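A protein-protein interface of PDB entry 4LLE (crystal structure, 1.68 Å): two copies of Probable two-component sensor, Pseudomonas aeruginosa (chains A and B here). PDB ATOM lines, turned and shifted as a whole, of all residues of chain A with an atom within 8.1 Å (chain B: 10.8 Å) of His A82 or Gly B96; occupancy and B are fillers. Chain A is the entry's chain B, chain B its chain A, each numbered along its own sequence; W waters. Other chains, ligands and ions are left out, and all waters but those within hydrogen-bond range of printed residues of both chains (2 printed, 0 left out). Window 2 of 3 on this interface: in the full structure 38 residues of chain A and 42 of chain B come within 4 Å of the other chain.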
ATOM      1  N   LEU A  32     -21.871  -8.283  -2.346  1.00  0.00           N
ATOM      2  CA  LEU A  32     -21.569  -8.705  -3.701  1.00  0.00           C
ATOM      3  C   LEU A  32     -21.857  -7.606  -4.732  1.00  0.00           C
ATOM      4  O   LEU A  32     -21.289  -7.608  -5.819  1.00  0.00           O
ATOM      5  CB  LEU A  32     -22.323 -10.003  -4.023  1.00  0.00           C
ATOM      6  CG  LEU A  32     -21.780 -11.248  -3.300  1.00  0.00           C
ATOM      7  CD1 LEU A  32     -22.739 -12.416  -3.432  1.00  0.00           C
ATOM      8  CD2 LEU A  32     -20.403 -11.640  -3.810  1.00  0.00           C
ATOM      9  N   ALA A  75     -30.391 -25.286  -0.815  1.00  0.00           N
ATOM     10  CA  ALA A  75     -30.403 -24.133  -1.708  1.00  0.00           C
ATOM     11  C   ALA A  75     -29.240 -23.191  -1.401  1.00  0.00           C
ATOM     12  O   ALA A  75     -28.668 -22.562  -2.300  1.00  0.00           O
ATOM     13  CB  ALA A  75     -31.726 -23.383  -1.596  1.00  0.00           C
ATOM     14  N   TYR A  76     -28.906 -23.074  -0.126  1.00  0.00           N
ATOM     15  CA  TYR A  76     -27.830 -22.184   0.268  1.00  0.00           C
ATOM     16  C   TYR A  76     -26.505 -22.771  -0.196  1.00  0.00           C
ATOM     17  O   TYR A  76     -25.610 -22.036  -0.601  1.00  0.00           O
ATOM     18  CB  TYR A  76     -27.803 -21.968   1.770  1.00  0.00           C
ATOM     19  CG  TYR A  76     -26.895 -20.829   2.138  1.00  0.00           C
ATOM     20  CD1 TYR A  76     -27.182 -19.549   1.703  1.00  0.00           C
ATOM     21  CD2 TYR A  76     -25.743 -21.031   2.893  1.00  0.00           C
ATOM     22  CE1 TYR A  76     -26.370 -18.483   2.017  1.00  0.00           C
ATOM     23  CE2 TYR A  76     -24.912 -19.954   3.223  1.00  0.00           C
ATOM     24  CZ  TYR A  76     -25.242 -18.685   2.775  1.00  0.00           C
ATOM     25  OH  TYR A  76     -24.454 -17.584   3.072  1.00  0.00           O
ATOM     26  N   LEU A  77     -26.417 -24.097  -0.159  1.00  0.00           N
ATOM     27  CA  LEU A  77     -25.262 -24.816  -0.704  1.00  0.00           C
ATOM     28  C   LEU A  77     -25.086 -24.525  -2.184  1.00  0.00           C
ATOM     29  O   LEU A  77     -23.967 -24.292  -2.646  1.00  0.00           O
ATOM     30  CB  LEU A  77     -25.428 -26.308  -0.481  1.00  0.00           C
ATOM     31  CG  LEU A  77     -25.563 -26.561   1.007  1.00  0.00           C
ATOM     32  CD1 LEU A  77     -25.847 -28.026   1.264  1.00  0.00           C
ATOM     33  CD2 LEU A  77     -24.295 -26.060   1.689  1.00  0.00           C
ATOM     34  N   GLN A  78     -26.191 -24.536  -2.924  1.00  0.00           N
ATOM     35  CA  GLN A  78     -26.132 -24.197  -4.340  1.00  0.00           C
ATOM     36  C   GLN A  78     -25.708 -22.748  -4.551  1.00  0.00           C
ATOM     37  O   GLN A  78     -24.900 -22.461  -5.441  1.00  0.00           O
ATOM     38  CB  GLN A  78     -27.456 -24.495  -5.040  1.00  0.00           C
ATOM     39  CG  GLN A  78     -27.594 -25.947  -5.444  1.00  0.00           C
ATOM     40  CD  GLN A  78     -26.361 -26.456  -6.164  1.00  0.00           C
ATOM     41  OE1 GLN A  78     -25.900 -25.852  -7.131  1.00  0.00           O
ATOM     42  NE2 GLN A  78     -25.818 -27.564  -5.689  1.00  0.00           N
ATOM     43  N   LEU A  79     -26.229 -21.833  -3.736  1.00  0.00           N
ATOM     44  CA  LEU A  79     -25.846 -20.427  -3.858  1.00  0.00           C
ATOM     45  C   LEU A  79     -24.342 -20.289  -3.677  1.00  0.00           C
ATOM     46  O   LEU A  79     -23.677 -19.578  -4.424  1.00  0.00           O
ATOM     47  CB  LEU A  79     -26.575 -19.561  -2.824  1.00  0.00           C
ATOM     48  CG  LEU A  79     -26.315 -18.060  -2.996  1.00  0.00           C
ATOM     49  CD1 LEU A  79     -26.915 -17.569  -4.306  1.00  0.00           C
ATOM     50  CD2 LEU A  79     -26.870 -17.273  -1.825  1.00  0.00           C
ATOM     51  N   GLN A  80     -23.811 -20.990  -2.684  1.00  0.00           N
ATOM     52  CA  GLN A  80     -22.370 -21.003  -2.437  1.00  0.00           C
ATOM     53  C   GLN A  80     -21.579 -21.568  -3.613  1.00  0.00           C
ATOM     54  O   GLN A  80     -20.537 -21.023  -3.991  1.00  0.00           O
ATOM     55  CB  GLN A  80     -22.062 -21.798  -1.171  1.00  0.00           C
ATOM     56  CG  GLN A  80     -22.305 -21.041   0.112  1.00  0.00           C
ATOM     57  CD  GLN A  80     -21.428 -21.546   1.239  1.00  0.00           C
ATOM     58  OE1 GLN A  80     -21.568 -22.683   1.692  1.00  0.00           O
ATOM     59  NE2 GLN A  80     -20.503 -20.705   1.689  1.00  0.00           N
ATOM     60  N   ALA A  81     -22.071 -22.661  -4.184  1.00  0.00           N
ATOM     61  CA  ALA A  81     -21.417 -23.297  -5.326  1.00  0.00           C
ATOM     62  C   ALA A  81     -21.243 -22.298  -6.470  1.00  0.00           C
ATOM     63  O   ALA A  81     -20.299 -22.385  -7.243  1.00  0.00           O
ATOM     64  CB  ALA A  81     -22.228 -24.501  -5.796  1.00  0.00           C
ATOM     65  N   HIS A  82     -22.158 -21.339  -6.561  1.00  0.00           N
ATOM     66  CA  HIS A  82     -22.158 -20.402  -7.677  1.00  0.00           C
ATOM     67  C   HIS A  82     -21.670 -19.019  -7.253  1.00  0.00           C
ATOM     68  O   HIS A  82     -21.798 -18.062  -8.014  1.00  0.00           O
ATOM     69  CB  HIS A  82     -23.567 -20.277  -8.268  1.00  0.00           C
ATOM     70  CG  HIS A  82     -24.011 -21.480  -9.039  1.00  0.00           C
ATOM     71  ND1 HIS A  82     -24.624 -22.564  -8.447  1.00  0.00           N
ATOM     72  CD2 HIS A  82     -23.920 -21.773 -10.359  1.00  0.00           C
ATOM     73  CE1 HIS A  82     -24.898 -23.469  -9.369  1.00  0.00           C
ATOM     74  NE2 HIS A  82     -24.480 -23.016 -10.538  1.00  0.00           N
ATOM     75  N   THR A  83     -21.132 -18.913  -6.042  1.00  0.00           N
ATOM     76  CA  THR A  83     -20.745 -17.608  -5.499  1.00  0.00           C
ATOM     77  C   THR A  83     -19.396 -17.137  -6.038  1.00  0.00           C
ATOM     78  O   THR A  83     -18.364 -17.751  -5.767  1.00  0.00           O
ATOM     79  CB  THR A  83     -20.734 -17.607  -3.959  1.00  0.00           C
ATOM     80  OG1 THR A  83     -22.076 -17.449  -3.476  1.00  0.00           O
ATOM     81  CG2 THR A  83     -19.879 -16.458  -3.423  1.00  0.00           C
ATOM     82  N   PRO A  84     -19.413 -16.050  -6.826  1.00  0.00           N
ATOM     83  CA  PRO A  84     -18.228 -15.429  -7.414  1.00  0.00           C
ATOM     84  C   PRO A  84     -17.829 -14.165  -6.656  1.00  0.00           C
ATOM     85  O   PRO A  84     -18.234 -14.002  -5.505  1.00  0.00           O
ATOM     86  CB  PRO A  84     -18.709 -15.064  -8.822  1.00  0.00           C
ATOM     87  CG  PRO A  84     -20.233 -14.915  -8.694  1.00  0.00           C
ATOM     88  CD  PRO A  84     -20.638 -15.399  -7.316  1.00  0.00           C
ATOM     89  N   LEU B  29     -33.606  -7.933  -8.544  1.00  0.00           N
ATOM     90  CA  LEU B  29     -32.246  -8.404  -8.340  1.00  0.00           C
ATOM     91  C   LEU B  29     -31.949  -9.610  -9.230  1.00  0.00           C
ATOM     92  O   LEU B  29     -30.870  -9.706  -9.805  1.00  0.00           O
ATOM     93  CB  LEU B  29     -32.030  -8.783  -6.879  1.00  0.00           C
ATOM     94  CG  LEU B  29     -32.044  -7.658  -5.852  1.00  0.00           C
ATOM     95  CD1 LEU B  29     -32.076  -8.262  -4.456  1.00  0.00           C
ATOM     96  CD2 LEU B  29     -30.849  -6.745  -6.035  1.00  0.00           C
ATOM     97  N   VAL B  30     -32.899 -10.542  -9.319  1.00  0.00           N
ATOM     98  CA  VAL B  30     -32.732 -11.720 -10.168  1.00  0.00           C
ATOM     99  C   VAL B  30     -32.398 -11.281 -11.586  1.00  0.00           C
ATOM    100  O   VAL B  30     -31.501 -11.834 -12.224  1.00  0.00           O
ATOM    101  CB  VAL B  30     -33.971 -12.651 -10.147  1.00  0.00           C
ATOM    102  CG1 VAL B  30     -33.901 -13.711 -11.258  1.00  0.00           C
ATOM    103  CG2 VAL B  30     -34.069 -13.340  -8.789  1.00  0.00           C
ATOM    104  N   ILE B  31     -33.109 -10.276 -12.070  1.00  0.00           N
ATOM    105  CA  ILE B  31     -32.892  -9.789 -13.433  1.00  0.00           C
ATOM    106  C   ILE B  31     -31.517  -9.153 -13.583  1.00  0.00           C
ATOM    107  O   ILE B  31     -30.819  -9.367 -14.580  1.00  0.00           O
ATOM    108  CB  ILE B  31     -33.967  -8.780 -13.840  1.00  0.00           C
ATOM    109  CG1 ILE B  31     -35.308  -9.482 -14.042  1.00  0.00           C
ATOM    110  CG2 ILE B  31     -33.580  -8.062 -15.129  1.00  0.00           C
ATOM    111  CD1 ILE B  31     -36.512  -8.557 -13.975  1.00  0.00           C
ATOM    112  N   LEU B  32     -31.140  -8.366 -12.584  1.00  0.00           N
ATOM    113  CA  LEU B  32     -29.891  -7.608 -12.612  1.00  0.00           C
ATOM    114  C   LEU B  32     -28.660  -8.495 -12.444  1.00  0.00           C
ATOM    115  O   LEU B  32     -27.558  -8.122 -12.851  1.00  0.00           O
ATOM    116  CB  LEU B  32     -29.914  -6.517 -11.526  1.00  0.00           C
ATOM    117  CG  LEU B  32     -30.861  -5.337 -11.799  1.00  0.00           C
ATOM    118  CD1 LEU B  32     -31.137  -4.507 -10.558  1.00  0.00           C
ATOM    119  CD2 LEU B  32     -30.327  -4.457 -12.928  1.00  0.00           C
ATOM    120  N   LEU B  33     -28.849  -9.665 -11.839  1.00  0.00           N
ATOM    121  CA  LEU B  33     -27.748 -10.586 -11.567  1.00  0.00           C
ATOM    122  C   LEU B  33     -27.418 -11.488 -12.750  1.00  0.00           C
ATOM    123  O   LEU B  33     -26.424 -12.227 -12.722  1.00  0.00           O
ATOM    124  CB  LEU B  33     -28.078 -11.445 -10.346  1.00  0.00           C
ATOM    125  CG  LEU B  33     -28.063 -10.706  -9.008  1.00  0.00           C
ATOM    126  CD1 LEU B  33     -28.565 -11.631  -7.915  1.00  0.00           C
ATOM    127  CD2 LEU B  33     -26.659 -10.208  -8.702  1.00  0.00           C
ATOM    128  N   ARG B  34     -28.249 -11.442 -13.787  1.00  0.00           N
ATOM    129  CA  ARG B  34     -27.999 -12.265 -14.966  1.00  0.00           C
ATOM    130  C   ARG B  34     -26.917 -11.621 -15.830  1.00  0.00           C
ATOM    131  O   ARG B  34     -26.650 -10.424 -15.711  1.00  0.00           O
ATOM    132  CB  ARG B  34     -29.289 -12.501 -15.749  1.00  0.00           C
ATOM    133  CG  ARG B  34     -30.310 -13.338 -14.962  1.00  0.00           C
ATOM    134  CD  ARG B  34     -31.496 -13.767 -15.804  1.00  0.00           C
ATOM    135  NE  ARG B  34     -31.101 -14.631 -16.919  1.00  0.00           N
ATOM    136  CZ  ARG B  34     -30.946 -15.949 -16.837  1.00  0.00           C
ATOM    137  NH1 ARG B  34     -30.587 -16.639 -17.909  1.00  0.00           N
ATOM    138  NH2 ARG B  34     -31.150 -16.582 -15.688  1.00  0.00           N
ATOM    139  N   GLU B  35     -26.273 -12.427 -16.672  1.00  0.00           N
ATOM    140  CA  GLU B  35     -25.166 -11.940 -17.493  1.00  0.00           C
ATOM    141  C   GLU B  35     -25.636 -10.867 -18.466  1.00  0.00           C
ATOM    142  O   GLU B  35     -24.925  -9.897 -18.737  1.00  0.00           O
ATOM    143  CB  GLU B  35     -24.502 -13.095 -18.249  1.00  0.00           C
ATOM    144  CG  GLU B  35     -23.848 -12.704 -19.577  1.00  0.00           C
ATOM    145  CD  GLU B  35     -22.591 -11.863 -19.418  1.00  0.00           C
ATOM    146  OE1 GLU B  35     -22.497 -11.090 -18.440  1.00  0.00           O
ATOM    147  OE2 GLU B  35     -21.691 -11.978 -20.278  1.00  0.00           O
ATOM    148  N   THR B  36     -26.842 -11.047 -18.991  1.00  0.00           N
ATOM    149  CA  THR B  36     -27.436 -10.060 -19.873  1.00  0.00           C
ATOM    150  C   THR B  36     -28.795  -9.625 -19.326  1.00  0.00           C
ATOM    151  O   THR B  36     -29.817 -10.191 -19.700  1.00  0.00           O
ATOM    152  CB  THR B  36     -27.604 -10.637 -21.291  1.00  0.00           C
ATOM    153  OG1 THR B  36     -26.334 -11.102 -21.765  1.00  0.00           O
ATOM    154  CG2 THR B  36     -28.147  -9.587 -22.250  1.00  0.00           C
ATOM    155  N   ALA B  92     -19.486  -9.666 -16.523  1.00  0.00           N
ATOM    156  CA  ALA B  92     -19.741 -11.025 -16.060  1.00  0.00           C
ATOM    157  C   ALA B  92     -20.686 -11.039 -14.858  1.00  0.00           C
ATOM    158  O   ALA B  92     -20.476 -10.316 -13.884  1.00  0.00           O
ATOM    159  CB  ALA B  92     -18.431 -11.725 -15.718  1.00  0.00           C
ATOM    160  N   ASP B  93     -21.725 -11.865 -14.939  1.00  0.00           N
ATOM    161  CA  ASP B  93     -22.674 -12.035 -13.843  1.00  0.00           C
ATOM    162  C   ASP B  93     -23.406 -13.367 -13.971  1.00  0.00           C
ATOM    163  O   ASP B  93     -24.369 -13.487 -14.725  1.00  0.00           O
ATOM    164  CB  ASP B  93     -23.678 -10.882 -13.803  1.00  0.00           C
ATOM    165  CG  ASP B  93     -23.186  -9.707 -12.981  1.00  0.00           C
ATOM    166  OD1 ASP B  93     -22.426  -9.933 -12.014  1.00  0.00           O
ATOM    167  OD2 ASP B  93     -23.560  -8.558 -13.301  1.00  0.00           O
ATOM    168  N   ASN B  94     -22.938 -14.358 -13.224  1.00  0.00           N
ATOM    169  CA  ASN B  94     -23.443 -15.723 -13.319  1.00  0.00           C
ATOM    170  C   ASN B  94     -24.968 -15.824 -13.477  1.00  0.00           C
ATOM    171  O   ASN B  94     -25.724 -15.339 -12.622  1.00  0.00           O
ATOM    172  CB  ASN B  94     -22.992 -16.519 -12.087  1.00  0.00           C
ATOM    173  CG  ASN B  94     -22.857 -18.003 -12.363  1.00  0.00           C
ATOM    174  OD1 ASN B  94     -23.328 -18.500 -13.386  1.00  0.00           O
ATOM    175  ND2 ASN B  94     -22.215 -18.721 -11.447  1.00  0.00           N
ATOM    176  N   ASP B  95     -25.417 -16.437 -14.573  1.00  0.00           N
ATOM    177  CA  ASP B  95     -26.812 -16.857 -14.663  1.00  0.00           C
ATOM    178  C   ASP B  95     -27.043 -17.853 -13.537  1.00  0.00           C
ATOM    179  O   ASP B  95     -28.084 -17.838 -12.879  1.00  0.00           O
ATOM    180  CB  ASP B  95     -27.125 -17.525 -16.003  1.00  0.00           C
ATOM    181  CG  ASP B  95     -27.282 -16.528 -17.139  1.00  0.00           C
ATOM    182  OD1 ASP B  95     -27.334 -15.310 -16.867  1.00  0.00           O
ATOM    183  OD2 ASP B  95     -27.390 -16.978 -18.304  1.00  0.00           O
ATOM    184  N   GLY B  96     -26.048 -18.708 -13.313  1.00  0.00           N
ATOM    185  CA  GLY B  96     -26.105 -19.702 -12.254  1.00  0.00           C
ATOM    186  C   GLY B  96     -26.302 -19.104 -10.870  1.00  0.00           C
ATOM    187  O   GLY B  96     -27.083 -19.622 -10.066  1.00  0.00           O
ATOM    188  N   PHE B  97     -25.593 -18.022 -10.576  1.00  0.00           N
ATOM    189  CA  PHE B  97     -25.791 -17.350  -9.303  1.00  0.00           C
ATOM    190  C   PHE B  97     -27.196 -16.769  -9.199  1.00  0.00           C
ATOM    191  O   PHE B  97     -27.864 -16.934  -8.177  1.00  0.00           O
ATOM    192  CB  PHE B  97     -24.774 -16.237  -9.087  1.00  0.00           C
ATOM    193  CG  PHE B  97     -24.943 -15.530  -7.778  1.00  0.00           C
ATOM    194  CD1 PHE B  97     -24.317 -16.001  -6.640  1.00  0.00           C
ATOM    195  CD2 PHE B  97     -25.756 -14.414  -7.679  1.00  0.00           C
ATOM    196  CE1 PHE B  97     -24.469 -15.362  -5.432  1.00  0.00           C
ATOM    197  CE2 PHE B  97     -25.930 -13.768  -6.467  1.00  0.00           C
ATOM    198  CZ  PHE B  97     -25.286 -14.245  -5.337  1.00  0.00           C
ATOM    199  N   SER B  98     -27.627 -16.051 -10.234  1.00  0.00           N
ATOM    200  CA  SER B  98     -28.985 -15.502 -10.244  1.00  0.00           C
ATOM    201  C   SER B  98     -30.042 -16.596  -9.986  1.00  0.00           C
ATOM    202  O   SER B  98     -30.980 -16.403  -9.213  1.00  0.00           O
ATOM    203  CB  SER B  98     -29.267 -14.833 -11.599  1.00  0.00           C
ATOM    204  OG  SER B  98     -30.626 -14.440 -11.698  1.00  0.00           O
ATOM    205  N   GLU B  99     -29.888 -17.746 -10.629  1.00  0.00           N
ATOM    206  CA  GLU B  99     -30.863 -18.833 -10.486  1.00  0.00           C
ATOM    207  C   GLU B  99     -30.843 -19.416  -9.070  1.00  0.00           C
ATOM    208  O   GLU B  99     -31.885 -19.712  -8.491  1.00  0.00           O
ATOM    209  CB  GLU B  99     -30.583 -19.955 -11.498  1.00  0.00           C
ATOM    210  CG  GLU B  99     -30.410 -19.487 -12.947  1.00  0.00           C
ATOM    211  CD  GLU B  99     -31.689 -19.555 -13.766  1.00  0.00           C
ATOM    212  OE1 GLU B  99     -32.778 -19.318 -13.203  1.00  0.00           O
ATOM    213  OE2 GLU B  99     -31.601 -19.850 -14.979  1.00  0.00           O
ATOM    214  N   ALA B 100     -29.650 -19.599  -8.520  1.00  0.00           N
ATOM    215  CA  ALA B 100     -29.541 -20.122  -7.157  1.00  0.00           C
ATOM    216  C   ALA B 100     -30.151 -19.154  -6.148  1.00  0.00           C
ATOM    217  O   ALA B 100     -30.849 -19.567  -5.208  1.00  0.00           O
ATOM    218  CB  ALA B 100     -28.078 -20.398  -6.802  1.00  0.00           C
ATOM    219  N   PHE B 101     -29.861 -17.872  -6.335  1.00  0.00           N
ATOM    220  CA  PHE B 101     -30.389 -16.839  -5.458  1.00  0.00           C
ATOM    221  C   PHE B 101     -31.908 -16.884  -5.500  1.00  0.00           C
ATOM    222  O   PHE B 101     -32.582 -16.852  -4.475  1.00  0.00           O
ATOM    223  CB  PHE B 101     -29.903 -15.456  -5.888  1.00  0.00           C
ATOM    224  CG  PHE B 101     -30.723 -14.337  -5.308  1.00  0.00           C
ATOM    225  CD1 PHE B 101     -30.694 -14.082  -3.951  1.00  0.00           C
ATOM    226  CD2 PHE B 101     -31.553 -13.574  -6.114  1.00  0.00           C
ATOM    227  CE1 PHE B 101     -31.467 -13.056  -3.413  1.00  0.00           C
ATOM    228  CE2 PHE B 101     -32.324 -12.552  -5.580  1.00  0.00           C
ATOM    229  CZ  PHE B 101     -32.278 -12.301  -4.224  1.00  0.00           C
ATOM    230  N   ASN B 102     -32.451 -16.972  -6.706  1.00  0.00           N
ATOM    231  CA  ASN B 102     -33.889 -16.978  -6.853  1.00  0.00           C
ATOM    232  C   ASN B 102     -34.540 -18.102  -6.047  1.00  0.00           C
ATOM    233  O   ASN B 102     -35.492 -17.887  -5.305  1.00  0.00           O
ATOM    234  CB  ASN B 102     -34.230 -17.134  -8.333  1.00  0.00           C
ATOM    235  CG  ASN B 102     -35.540 -16.494  -8.686  1.00  0.00           C
ATOM    236  OD1 ASN B 102     -36.202 -15.914  -7.841  1.00  0.00           O
ATOM    237  ND2 ASN B 102     -35.917 -16.592  -9.950  1.00  0.00           N
ATOM    238  N   GLY B 103     -34.020 -19.311  -6.202  1.00  0.00           N
ATOM    239  CA  GLY B 103     -34.578 -20.460  -5.512  1.00  0.00           C
ATOM    240  C   GLY B 103     -34.470 -20.319  -4.000  1.00  0.00           C
ATOM    241  O   GLY B 103     -35.415 -20.607  -3.272  1.00  0.00           O
ATOM    242  N   LEU B 104     -33.319 -19.865  -3.525  1.00  0.00           N
ATOM    243  CA  LEU B 104     -33.139 -19.692  -2.085  1.00  0.00           C
ATOM    244  C   LEU B 104     -34.098 -18.659  -1.497  1.00  0.00           C
ATOM    245  O   LEU B 104     -34.725 -18.892  -0.464  1.00  0.00           O
ATOM    246  CB  LEU B 104     -31.702 -19.299  -1.768  1.00  0.00           C
ATOM    247  CG  LEU B 104     -31.425 -18.921  -0.310  1.00  0.00           C
ATOM    248  CD1 LEU B 104     -31.701 -20.127   0.651  1.00  0.00           C
ATOM    249  CD2 LEU B 104     -29.980 -18.458  -0.211  1.00  0.00           C
HETATM  250  O   HOH W   1     -30.389 -22.213  -4.527  1.00  0.00           O
HETATM  251  O   HOH W   2     -27.755 -22.159  -9.847  1.00  0.00           O
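The side-chain amide oxygen (OD1) of Asn B94 is in hydrogen-bond range of the backbone NH (N) of Gly B96 (2.7 Å). The backbone carbonyl oxygen (O) of Leu A79 is in hydrogen-bond range of the side-chain hydroxyl (OG1) of Thr A83 (2.8 Å). O of Gln A78 is in hydrogen-bond range of ND1 of His A82 (3.0 Å).
Among the printed residues, merely in contact across the chains: Leu A79 with Phe B97, His A82 with Asn B94, His A82 with Phe B97, His A82 with Gly B96, Tyr A76 with Leu B104, Leu A79 with Phe B101, Leu A32 with Phe B97, Leu A79 with Ala B100, Leu A79 with Leu B104, Thr A83 with Phe B97, Pro A84 with Phe B97 and Ala A75 with Leu B104.
Of the printed residues of chain B, Leu A32 touches Phe B97 (3.7 Å). Of the printed residues of chain B, Tyr A76 touches Leu B104. No residue of chain B comes within 4 Å of Ala A81. Of chain B, only Asn B94 (3.5 Å), Gly B96 (3.6 Å) and Phe B97 (3.5 Å) come within 4 Å of His A82. Of the printed residues of chain B, Thr A83 touches Phe B97 (3.7 Å). Leu B33 touches none of the printed residues of chain A. Of chain A, only His A82 (3.6 Å) comes within 4 Å of Gly B96. Printed residues of chain A within 4 Å of Leu B104: Ala A75, Tyr A76 and Leu A79.
Printed residues of chain A that touch a printed residue of chain B: Leu A32, Ala A75, Tyr A76, Leu A79, His A82, Thr A83 and Pro A84. Hydrophobic or aromatic side chains of chain B that line the printed part of chain A: Phe B97, Ala B100, Phe B101 and Leu B104. Among the printed residues, no Asp or Glu carboxylate lies within 4 Å of a Lys or Arg side-chain nitrogen of the other chain.
1 position is printed for both chains. Of the 12 pairs that touch across the chains among the printed residues, none has its exchanged pair printed and touching as well.
Water W2 lies within hydrogen-bond range of the backbone carbonyl oxygen (O) of Gly B96 (2.6 Å), the backbone NH (N) of Ala B100 (3.5 Å) and a ring nitrogen (ND1) of His A82 (3.5 Å). Water W1 bridges the backbone carbonyl oxygen of Ala B100 (2.8 Å) and the backbone carbonyl oxygen of Ala A75 (2.8 Å).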
